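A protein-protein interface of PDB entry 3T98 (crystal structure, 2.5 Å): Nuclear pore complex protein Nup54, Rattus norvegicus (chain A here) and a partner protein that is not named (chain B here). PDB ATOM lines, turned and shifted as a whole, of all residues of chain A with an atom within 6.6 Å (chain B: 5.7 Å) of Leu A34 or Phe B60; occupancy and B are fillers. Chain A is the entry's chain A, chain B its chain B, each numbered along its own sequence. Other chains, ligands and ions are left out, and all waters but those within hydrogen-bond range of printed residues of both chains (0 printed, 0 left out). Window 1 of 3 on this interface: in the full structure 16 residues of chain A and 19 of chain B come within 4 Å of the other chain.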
ATOM      1  N   HIS A  26     -25.615 -10.069 -16.009  1.00  0.00           N
ATOM      2  CA  HIS A  26     -24.838  -9.362 -15.012  1.00  0.00           C
ATOM      3  C   HIS A  26     -23.396  -9.198 -15.472  1.00  0.00           C
ATOM      4  O   HIS A  26     -22.812  -8.115 -15.386  1.00  0.00           O
ATOM      5  CB  HIS A  26     -24.853 -10.133 -13.701  1.00  0.00           C
ATOM      6  CG  HIS A  26     -24.109  -9.454 -12.600  1.00  0.00           C
ATOM      7  ND1 HIS A  26     -24.589  -8.329 -11.962  1.00  0.00           N
ATOM      8  CD2 HIS A  26     -22.900  -9.715 -12.048  1.00  0.00           C
ATOM      9  CE1 HIS A  26     -23.707  -7.924 -11.064  1.00  0.00           C
ATOM     10  NE2 HIS A  26     -22.673  -8.749 -11.096  1.00  0.00           N
ATOM     11  N   GLN A  29     -23.070  -6.544 -18.133  1.00  0.00           N
ATOM     12  CA  GLN A  29     -23.080  -5.197 -17.586  1.00  0.00           C
ATOM     13  C   GLN A  29     -21.701  -4.851 -17.024  1.00  0.00           C
ATOM     14  O   GLN A  29     -21.183  -3.753 -17.253  1.00  0.00           O
ATOM     15  CB  GLN A  29     -24.150  -5.085 -16.510  1.00  0.00           C
ATOM     16  CG  GLN A  29     -25.516  -5.533 -17.015  1.00  0.00           C
ATOM     17  CD  GLN A  29     -26.623  -5.207 -16.044  1.00  0.00           C
ATOM     18  OE1 GLN A  29     -26.353  -4.911 -14.886  1.00  0.00           O
ATOM     19  NE2 GLN A  29     -27.879  -5.276 -16.502  1.00  0.00           N
ATOM     20  N   GLN A  30     -21.099  -5.788 -16.294  1.00  0.00           N
ATOM     21  CA  GLN A  30     -19.761  -5.576 -15.742  1.00  0.00           C
ATOM     22  C   GLN A  30     -18.800  -5.252 -16.878  1.00  0.00           C
ATOM     23  O   GLN A  30     -17.968  -4.364 -16.761  1.00  0.00           O
ATOM     24  CB  GLN A  30     -19.252  -6.829 -15.027  1.00  0.00           C
ATOM     25  CG  GLN A  30     -19.846  -7.092 -13.661  1.00  0.00           C
ATOM     26  CD  GLN A  30     -19.129  -8.234 -12.932  1.00  0.00           C
ATOM     27  OE1 GLN A  30     -19.630  -8.765 -11.945  1.00  0.00           O
ATOM     28  NE2 GLN A  30     -17.946  -8.602 -13.416  1.00  0.00           N
ATOM     29  N   GLN A  31     -18.911  -6.003 -17.967  1.00  0.00           N
ATOM     30  CA  GLN A  31     -18.063  -5.805 -19.122  1.00  0.00           C
ATOM     31  C   GLN A  31     -18.295  -4.406 -19.702  1.00  0.00           C
ATOM     32  O   GLN A  31     -17.348  -3.645 -19.908  1.00  0.00           O
ATOM     33  CB  GLN A  31     -18.376  -6.868 -20.173  1.00  0.00           C
ATOM     34  CG  GLN A  31     -17.558  -6.752 -21.444  1.00  0.00           C
ATOM     35  CD  GLN A  31     -18.072  -7.675 -22.541  1.00  0.00           C
ATOM     36  OE1 GLN A  31     -19.278  -7.702 -22.833  1.00  0.00           O
ATOM     37  NE2 GLN A  31     -17.162  -8.433 -23.165  1.00  0.00           N
ATOM     38  N   GLU A  32     -19.554  -4.077 -19.973  1.00  0.00           N
ATOM     39  CA  GLU A  32     -19.908  -2.765 -20.505  1.00  0.00           C
ATOM     40  C   GLU A  32     -19.375  -1.678 -19.568  1.00  0.00           C
ATOM     41  O   GLU A  32     -18.926  -0.619 -20.019  1.00  0.00           O
ATOM     42  CB  GLU A  32     -21.429  -2.627 -20.621  1.00  0.00           C
ATOM     43  CG  GLU A  32     -22.083  -3.652 -21.539  1.00  0.00           C
ATOM     44  CD  GLU A  32     -23.590  -3.458 -21.658  1.00  0.00           C
ATOM     45  OE1 GLU A  32     -24.270  -3.400 -20.601  1.00  0.00           O
ATOM     46  OE2 GLU A  32     -24.091  -3.367 -22.806  1.00  0.00           O
ATOM     47  N   GLY A  33     -19.438  -1.947 -18.263  1.00  0.00           N
ATOM     48  CA  GLY A  33     -18.945  -0.998 -17.289  1.00  0.00           C
ATOM     49  C   GLY A  33     -17.475  -0.716 -17.523  1.00  0.00           C
ATOM     50  O   GLY A  33     -17.094   0.427 -17.768  1.00  0.00           O
ATOM     51  N   LEU A  34     -16.643  -1.754 -17.463  1.00  0.00           N
ATOM     52  CA  LEU A  34     -15.205  -1.602 -17.665  1.00  0.00           C
ATOM     53  C   LEU A  34     -14.831  -0.997 -19.025  1.00  0.00           C
ATOM     54  O   LEU A  34     -13.925  -0.168 -19.104  1.00  0.00           O
ATOM     55  CB  LEU A  34     -14.508  -2.957 -17.471  1.00  0.00           C
ATOM     56  CG  LEU A  34     -14.731  -3.616 -16.093  1.00  0.00           C
ATOM     57  CD1 LEU A  34     -14.159  -5.021 -16.119  1.00  0.00           C
ATOM     58  CD2 LEU A  34     -14.089  -2.800 -14.972  1.00  0.00           C
ATOM     59  N   SER A  35     -15.523  -1.411 -20.083  1.00  0.00           N
ATOM     60  CA  SER A  35     -15.272  -0.889 -21.432  1.00  0.00           C
ATOM     61  C   SER A  35     -15.558   0.607 -21.507  1.00  0.00           C
ATOM     62  O   SER A  35     -14.851   1.332 -22.195  1.00  0.00           O
ATOM     63  CB  SER A  35     -16.140  -1.595 -22.478  1.00  0.00           C
ATOM     64  OG  SER A  35     -15.890  -2.984 -22.508  1.00  0.00           O
ATOM     65  N   HIS A  36     -16.598   1.064 -20.810  1.00  0.00           N
ATOM     66  CA  HIS A  36     -16.919   2.477 -20.815  1.00  0.00           C
ATOM     67  C   HIS A  36     -15.771   3.296 -20.227  1.00  0.00           C
ATOM     68  O   HIS A  36     -15.422   4.358 -20.754  1.00  0.00           O
ATOM     69  CB  HIS A  36     -18.180   2.773 -20.018  1.00  0.00           C
ATOM     70  CG  HIS A  36     -18.652   4.185 -20.175  1.00  0.00           C
ATOM     71  ND1 HIS A  36     -18.905   5.016 -19.103  1.00  0.00           N
ATOM     72  CD2 HIS A  36     -18.880   4.925 -21.286  1.00  0.00           C
ATOM     73  CE1 HIS A  36     -19.267   6.206 -19.546  1.00  0.00           C
ATOM     74  NE2 HIS A  36     -19.260   6.177 -20.870  1.00  0.00           N
ATOM     75  N   LEU A  37     -15.202   2.804 -19.128  1.00  0.00           N
ATOM     76  CA  LEU A  37     -14.074   3.457 -18.467  1.00  0.00           C
ATOM     77  C   LEU A  37     -12.843   3.463 -19.390  1.00  0.00           C
ATOM     78  O   LEU A  37     -12.145   4.466 -19.493  1.00  0.00           O
ATOM     79  CB  LEU A  37     -13.754   2.738 -17.146  1.00  0.00           C
ATOM     80  CG  LEU A  37     -14.836   2.793 -16.055  1.00  0.00           C
ATOM     81  CD1 LEU A  37     -14.401   1.960 -14.856  1.00  0.00           C
ATOM     82  CD2 LEU A  37     -15.091   4.231 -15.634  1.00  0.00           C
ATOM     83  N   ILE A  38     -12.579   2.338 -20.050  1.00  0.00           N
ATOM     84  CA  ILE A  38     -11.458   2.228 -20.994  1.00  0.00           C
ATOM     85  C   ILE A  38     -11.671   3.285 -22.105  1.00  0.00           C
ATOM     86  O   ILE A  38     -10.730   3.984 -22.503  1.00  0.00           O
ATOM     87  CB  ILE A  38     -11.437   0.839 -21.678  1.00  0.00           C
ATOM     88  CG1 ILE A  38     -11.422  -0.282 -20.625  1.00  0.00           C
ATOM     89  CG2 ILE A  38     -10.274   0.756 -22.643  1.00  0.00           C
ATOM     90  CD1 ILE A  38     -10.060  -0.633 -20.068  1.00  0.00           C
ATOM     91  N   SER A  39     -12.910   3.367 -22.601  1.00  0.00           N
ATOM     92  CA  SER A  39     -13.320   4.313 -23.645  1.00  0.00           C
ATOM     93  C   SER A  39     -12.890   5.706 -23.270  1.00  0.00           C
ATOM     94  O   SER A  39     -12.183   6.375 -24.023  1.00  0.00           O
ATOM     95  CB  SER A  39     -14.849   4.334 -23.802  1.00  0.00           C
ATOM     96  OG  SER A  39     -15.325   3.266 -24.605  1.00  0.00           O
ATOM     97  N   TYR B  24      -9.313 -10.715 -12.398  1.00  0.00           N
ATOM     98  CA  TYR B  24     -10.602 -10.709 -13.075  1.00  0.00           C
ATOM     99  C   TYR B  24     -10.592 -11.675 -14.260  1.00  0.00           C
ATOM    100  O   TYR B  24     -11.508 -12.470 -14.429  1.00  0.00           O
ATOM    101  CB  TYR B  24     -10.905  -9.300 -13.580  1.00  0.00           C
ATOM    102  CG  TYR B  24     -12.303  -9.115 -14.110  1.00  0.00           C
ATOM    103  CD1 TYR B  24     -13.373  -8.915 -13.243  1.00  0.00           C
ATOM    104  CD2 TYR B  24     -12.556  -9.120 -15.481  1.00  0.00           C
ATOM    105  CE1 TYR B  24     -14.665  -8.716 -13.724  1.00  0.00           C
ATOM    106  CE2 TYR B  24     -13.847  -8.922 -15.980  1.00  0.00           C
ATOM    107  CZ  TYR B  24     -14.898  -8.719 -15.097  1.00  0.00           C
ATOM    108  OH  TYR B  24     -16.179  -8.499 -15.576  1.00  0.00           O
ATOM    109  N   LYS B  55     -16.654 -13.230  -5.679  1.00  0.00           N
ATOM    110  CA  LYS B  55     -15.239 -13.031  -5.959  1.00  0.00           C
ATOM    111  C   LYS B  55     -15.090 -12.134  -7.187  1.00  0.00           C
ATOM    112  O   LYS B  55     -14.315 -11.184  -7.181  1.00  0.00           O
ATOM    113  CB  LYS B  55     -14.546 -14.376  -6.216  1.00  0.00           C
ATOM    114  CG  LYS B  55     -14.581 -15.357  -5.054  1.00  0.00           C
ATOM    115  CD  LYS B  55     -13.758 -14.891  -3.868  1.00  0.00           C
ATOM    116  CE  LYS B  55     -13.726 -15.968  -2.783  1.00  0.00           C
ATOM    117  NZ  LYS B  55     -12.790 -15.667  -1.658  1.00  0.00           N
ATOM    118  N   ILE B  56     -15.852 -12.440  -8.231  1.00  0.00           N
ATOM    119  CA  ILE B  56     -15.805 -11.673  -9.468  1.00  0.00           C
ATOM    120  C   ILE B  56     -16.271 -10.228  -9.329  1.00  0.00           C
ATOM    121  O   ILE B  56     -15.635  -9.323  -9.847  1.00  0.00           O
ATOM    122  CB  ILE B  56     -16.629 -12.361 -10.568  1.00  0.00           C
ATOM    123  CG1 ILE B  56     -15.972 -13.691 -10.929  1.00  0.00           C
ATOM    124  CG2 ILE B  56     -16.729 -11.466 -11.786  1.00  0.00           C
ATOM    125  CD1 ILE B  56     -16.728 -14.511 -11.959  1.00  0.00           C
ATOM    126  N   TYR B  57     -17.376 -10.006  -8.633  1.00  0.00           N
ATOM    127  CA  TYR B  57     -17.886  -8.655  -8.467  1.00  0.00           C
ATOM    128  C   TYR B  57     -16.932  -7.798  -7.628  1.00  0.00           C
ATOM    129  O   TYR B  57     -16.871  -6.571  -7.792  1.00  0.00           O
ATOM    130  CB  TYR B  57     -19.260  -8.693  -7.810  1.00  0.00           C
ATOM    131  CG  TYR B  57     -19.915  -7.343  -7.724  1.00  0.00           C
ATOM    132  CD1 TYR B  57     -20.499  -6.757  -8.842  1.00  0.00           C
ATOM    133  CD2 TYR B  57     -19.948  -6.644  -6.520  1.00  0.00           C
ATOM    134  CE1 TYR B  57     -21.109  -5.502  -8.763  1.00  0.00           C
ATOM    135  CE2 TYR B  57     -20.551  -5.391  -6.428  1.00  0.00           C
ATOM    136  CZ  TYR B  57     -21.129  -4.826  -7.550  1.00  0.00           C
ATOM    137  OH  TYR B  57     -21.735  -3.595  -7.446  1.00  0.00           O
ATOM    138  N   GLN B  58     -16.195  -8.445  -6.730  1.00  0.00           N
ATOM    139  CA  GLN B  58     -15.238  -7.739  -5.887  1.00  0.00           C
ATOM    140  C   GLN B  58     -14.056  -7.231  -6.723  1.00  0.00           C
ATOM    141  O   GLN B  58     -13.587  -6.105  -6.527  1.00  0.00           O
ATOM    142  CB  GLN B  58     -14.760  -8.660  -4.757  1.00  0.00           C
ATOM    143  CG  GLN B  58     -15.689  -8.637  -3.536  1.00  0.00           C
ATOM    144  CD  GLN B  58     -15.610  -9.903  -2.685  1.00  0.00           C
ATOM    145  OE1 GLN B  58     -14.519 -10.359  -2.324  1.00  0.00           O
ATOM    146  NE2 GLN B  58     -16.773 -10.471  -2.355  1.00  0.00           N
ATOM    147  N   THR B  59     -13.587  -8.063  -7.654  1.00  0.00           N
ATOM    148  CA  THR B  59     -12.489  -7.697  -8.538  1.00  0.00           C
ATOM    149  C   THR B  59     -12.963  -6.560  -9.448  1.00  0.00           C
ATOM    150  O   THR B  59     -12.267  -5.548  -9.614  1.00  0.00           O
ATOM    151  CB  THR B  59     -12.065  -8.875  -9.427  1.00  0.00           C
ATOM    152  OG1 THR B  59     -11.716  -9.991  -8.607  1.00  0.00           O
ATOM    153  CG2 THR B  59     -10.866  -8.497 -10.278  1.00  0.00           C
ATOM    154  N   PHE B  60     -14.147  -6.742 -10.031  1.00  0.00           N
ATOM    155  CA  PHE B  60     -14.749  -5.752 -10.910  1.00  0.00           C
ATOM    156  C   PHE B  60     -14.713  -4.404 -10.220  1.00  0.00           C
ATOM    157  O   PHE B  60     -14.235  -3.423 -10.783  1.00  0.00           O
ATOM    158  CB  PHE B  60     -16.197  -6.132 -11.219  1.00  0.00           C
ATOM    159  CG  PHE B  60     -17.016  -5.009 -11.804  1.00  0.00           C
ATOM    160  CD1 PHE B  60     -16.927  -4.685 -13.153  1.00  0.00           C
ATOM    161  CD2 PHE B  60     -17.878  -4.268 -10.994  1.00  0.00           C
ATOM    162  CE1 PHE B  60     -17.694  -3.629 -13.697  1.00  0.00           C
ATOM    163  CE2 PHE B  60     -18.642  -3.221 -11.517  1.00  0.00           C
ATOM    164  CZ  PHE B  60     -18.550  -2.899 -12.876  1.00  0.00           C
ATOM    165  N   VAL B  61     -15.213  -4.361  -8.992  1.00  0.00           N
ATOM    166  CA  VAL B  61     -15.234  -3.114  -8.238  1.00  0.00           C
ATOM    167  C   VAL B  61     -13.845  -2.498  -8.056  1.00  0.00           C
ATOM    168  O   VAL B  61     -13.684  -1.277  -8.183  1.00  0.00           O
ATOM    169  CB  VAL B  61     -15.887  -3.316  -6.863  1.00  0.00           C
ATOM    170  CG1 VAL B  61     -15.685  -2.081  -5.999  1.00  0.00           C
ATOM    171  CG2 VAL B  61     -17.373  -3.585  -7.041  1.00  0.00           C
ATOM    172  N   ALA B  62     -12.849  -3.337  -7.766  1.00  0.00           N
ATOM    173  CA  ALA B  62     -11.479  -2.860  -7.576  1.00  0.00           C
ATOM    174  C   ALA B  62     -10.864  -2.439  -8.919  1.00  0.00           C
ATOM    175  O   ALA B  62     -10.106  -1.466  -8.997  1.00  0.00           O
ATOM    176  CB  ALA B  62     -10.618  -3.955  -6.918  1.00  0.00           C
ATOM    177  N   LEU B  63     -11.198  -3.182  -9.969  1.00  0.00           N
ATOM    178  CA  LEU B  63     -10.693  -2.908 -11.312  1.00  0.00           C
ATOM    179  C   LEU B  63     -11.287  -1.590 -11.809  1.00  0.00           C
ATOM    180  O   LEU B  63     -10.593  -0.737 -12.372  1.00  0.00           O
ATOM    181  CB  LEU B  63     -11.091  -4.055 -12.244  1.00  0.00           C
ATOM    182  CG  LEU B  63     -10.285  -4.277 -13.513  1.00  0.00           C
ATOM    183  CD1 LEU B  63      -8.790  -4.311 -13.201  1.00  0.00           C
ATOM    184  CD2 LEU B  63     -10.724  -5.584 -14.138  1.00  0.00           C
ATOM    185  N   ALA B  64     -12.584  -1.433 -11.586  1.00  0.00           N
ATOM    186  CA  ALA B  64     -13.282  -0.231 -11.992  1.00  0.00           C
ATOM    187  C   ALA B  64     -12.694   0.974 -11.261  1.00  0.00           C
ATOM    188  O   ALA B  64     -12.718   2.092 -11.772  1.00  0.00           O
ATOM    189  CB  ALA B  64     -14.771  -0.364 -11.684  1.00  0.00           C
ATOM    190  N   ALA B  65     -12.170   0.745 -10.062  1.00  0.00           N
ATOM    191  CA  ALA B  65     -11.582   1.827  -9.287  1.00  0.00           C
ATOM    192  C   ALA B  65     -10.244   2.205  -9.911  1.00  0.00           C
ATOM    193  O   ALA B  65      -9.919   3.378 -10.050  1.00  0.00           O
ATOM    194  CB  ALA B  65     -11.389   1.390  -7.826  1.00  0.00           C
ATOM    195  N   LEU B  67      -9.320   1.774 -13.018  1.00  0.00           N
ATOM    196  CA  LEU B  67      -9.511   2.415 -14.314  1.00  0.00           C
ATOM    197  C   LEU B  67      -9.890   3.860 -14.081  1.00  0.00           C
ATOM    198  O   LEU B  67      -9.471   4.748 -14.816  1.00  0.00           O
ATOM    199  CB  LEU B  67     -10.620   1.733 -15.112  1.00  0.00           C
ATOM    200  CG  LEU B  67     -10.252   0.401 -15.764  1.00  0.00           C
ATOM    201  CD1 LEU B  67     -11.507  -0.287 -16.244  1.00  0.00           C
ATOM    202  CD2 LEU B  67      -9.273   0.639 -16.899  1.00  0.00           C
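Printed residues of chain B that touch a printed residue of chain A: Tyr B24, Ile B56, Tyr B57, Phe B60, Ala B64 and Leu B67.
Hydrophobic or aromatic side chains of chain B that line the printed part of chain A: Tyr B24, Ile B56, Tyr B57, Phe B60, Ala B64 and Leu B67.
Along chain A the printed residues that touch a printed residue of chain B span positions 26 to 38.
Among the printed residues, 12 pairs touch across the chains.
OE1 of Gln A30 sits at hydrogen-bond distance from NE2 of His A26, at 3.2 Å.
Of the printed residues of chain B, Gln A30 touches Tyr B24 (2.8 Å), Ile B56 (3.5 Å), Tyr B57 (3.8 Å) and Phe B60 (3.2 Å).
Gln A31 touches none of the printed residues of chain B.
Printed residues of chain B within 4 Å of Leu A34: Tyr B24, Phe B60, Ala B64 and Leu B67.
Printed residues of chain A within 4 Å of Tyr B24: Gln A30 (2.8 Å) and Leu A34 (3.9 Å).
Of the printed residues of chain A, Tyr B57 touches His A26 and Gln A30.
Phe B60 touches just these residues of chain A: Gln A30 and Leu A34.
Printed residues of chain A within 4 Å of Ala B64: Leu A34 and Leu A37.
Printed residues of chain A within 4 Å of Leu B67: Leu A34 (3.7 Å), Leu A37 (3.8 Å) and Ile A38 (3.5 Å).
The nearest printed residue of chain B that does not touch Leu A34 is Leu B63 (4.01 Å).
The nearest residue of chain A that does not touch Phe B60 is Gly A33 (4.6 Å).
The side-chain hydroxyl (OH) of Tyr B24 lies within hydrogen-bond range of the side-chain amide nitrogen (NE2) of Gln A30, at 2.8 Å.
Among the printed residues, merely in contact across the chains: Gln A30 with Phe B60, Ile A38 with Leu B67, Gln A30 with Ile B56, Leu A37 with Ala B64, His A26 with Tyr B57, Leu A34 with Leu B67, Leu A37 with Leu B67, Gln A30 with Tyr B57, Leu A34 with Phe B60, Leu A34 with Tyr B24 and Leu A34 with Ala B64.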
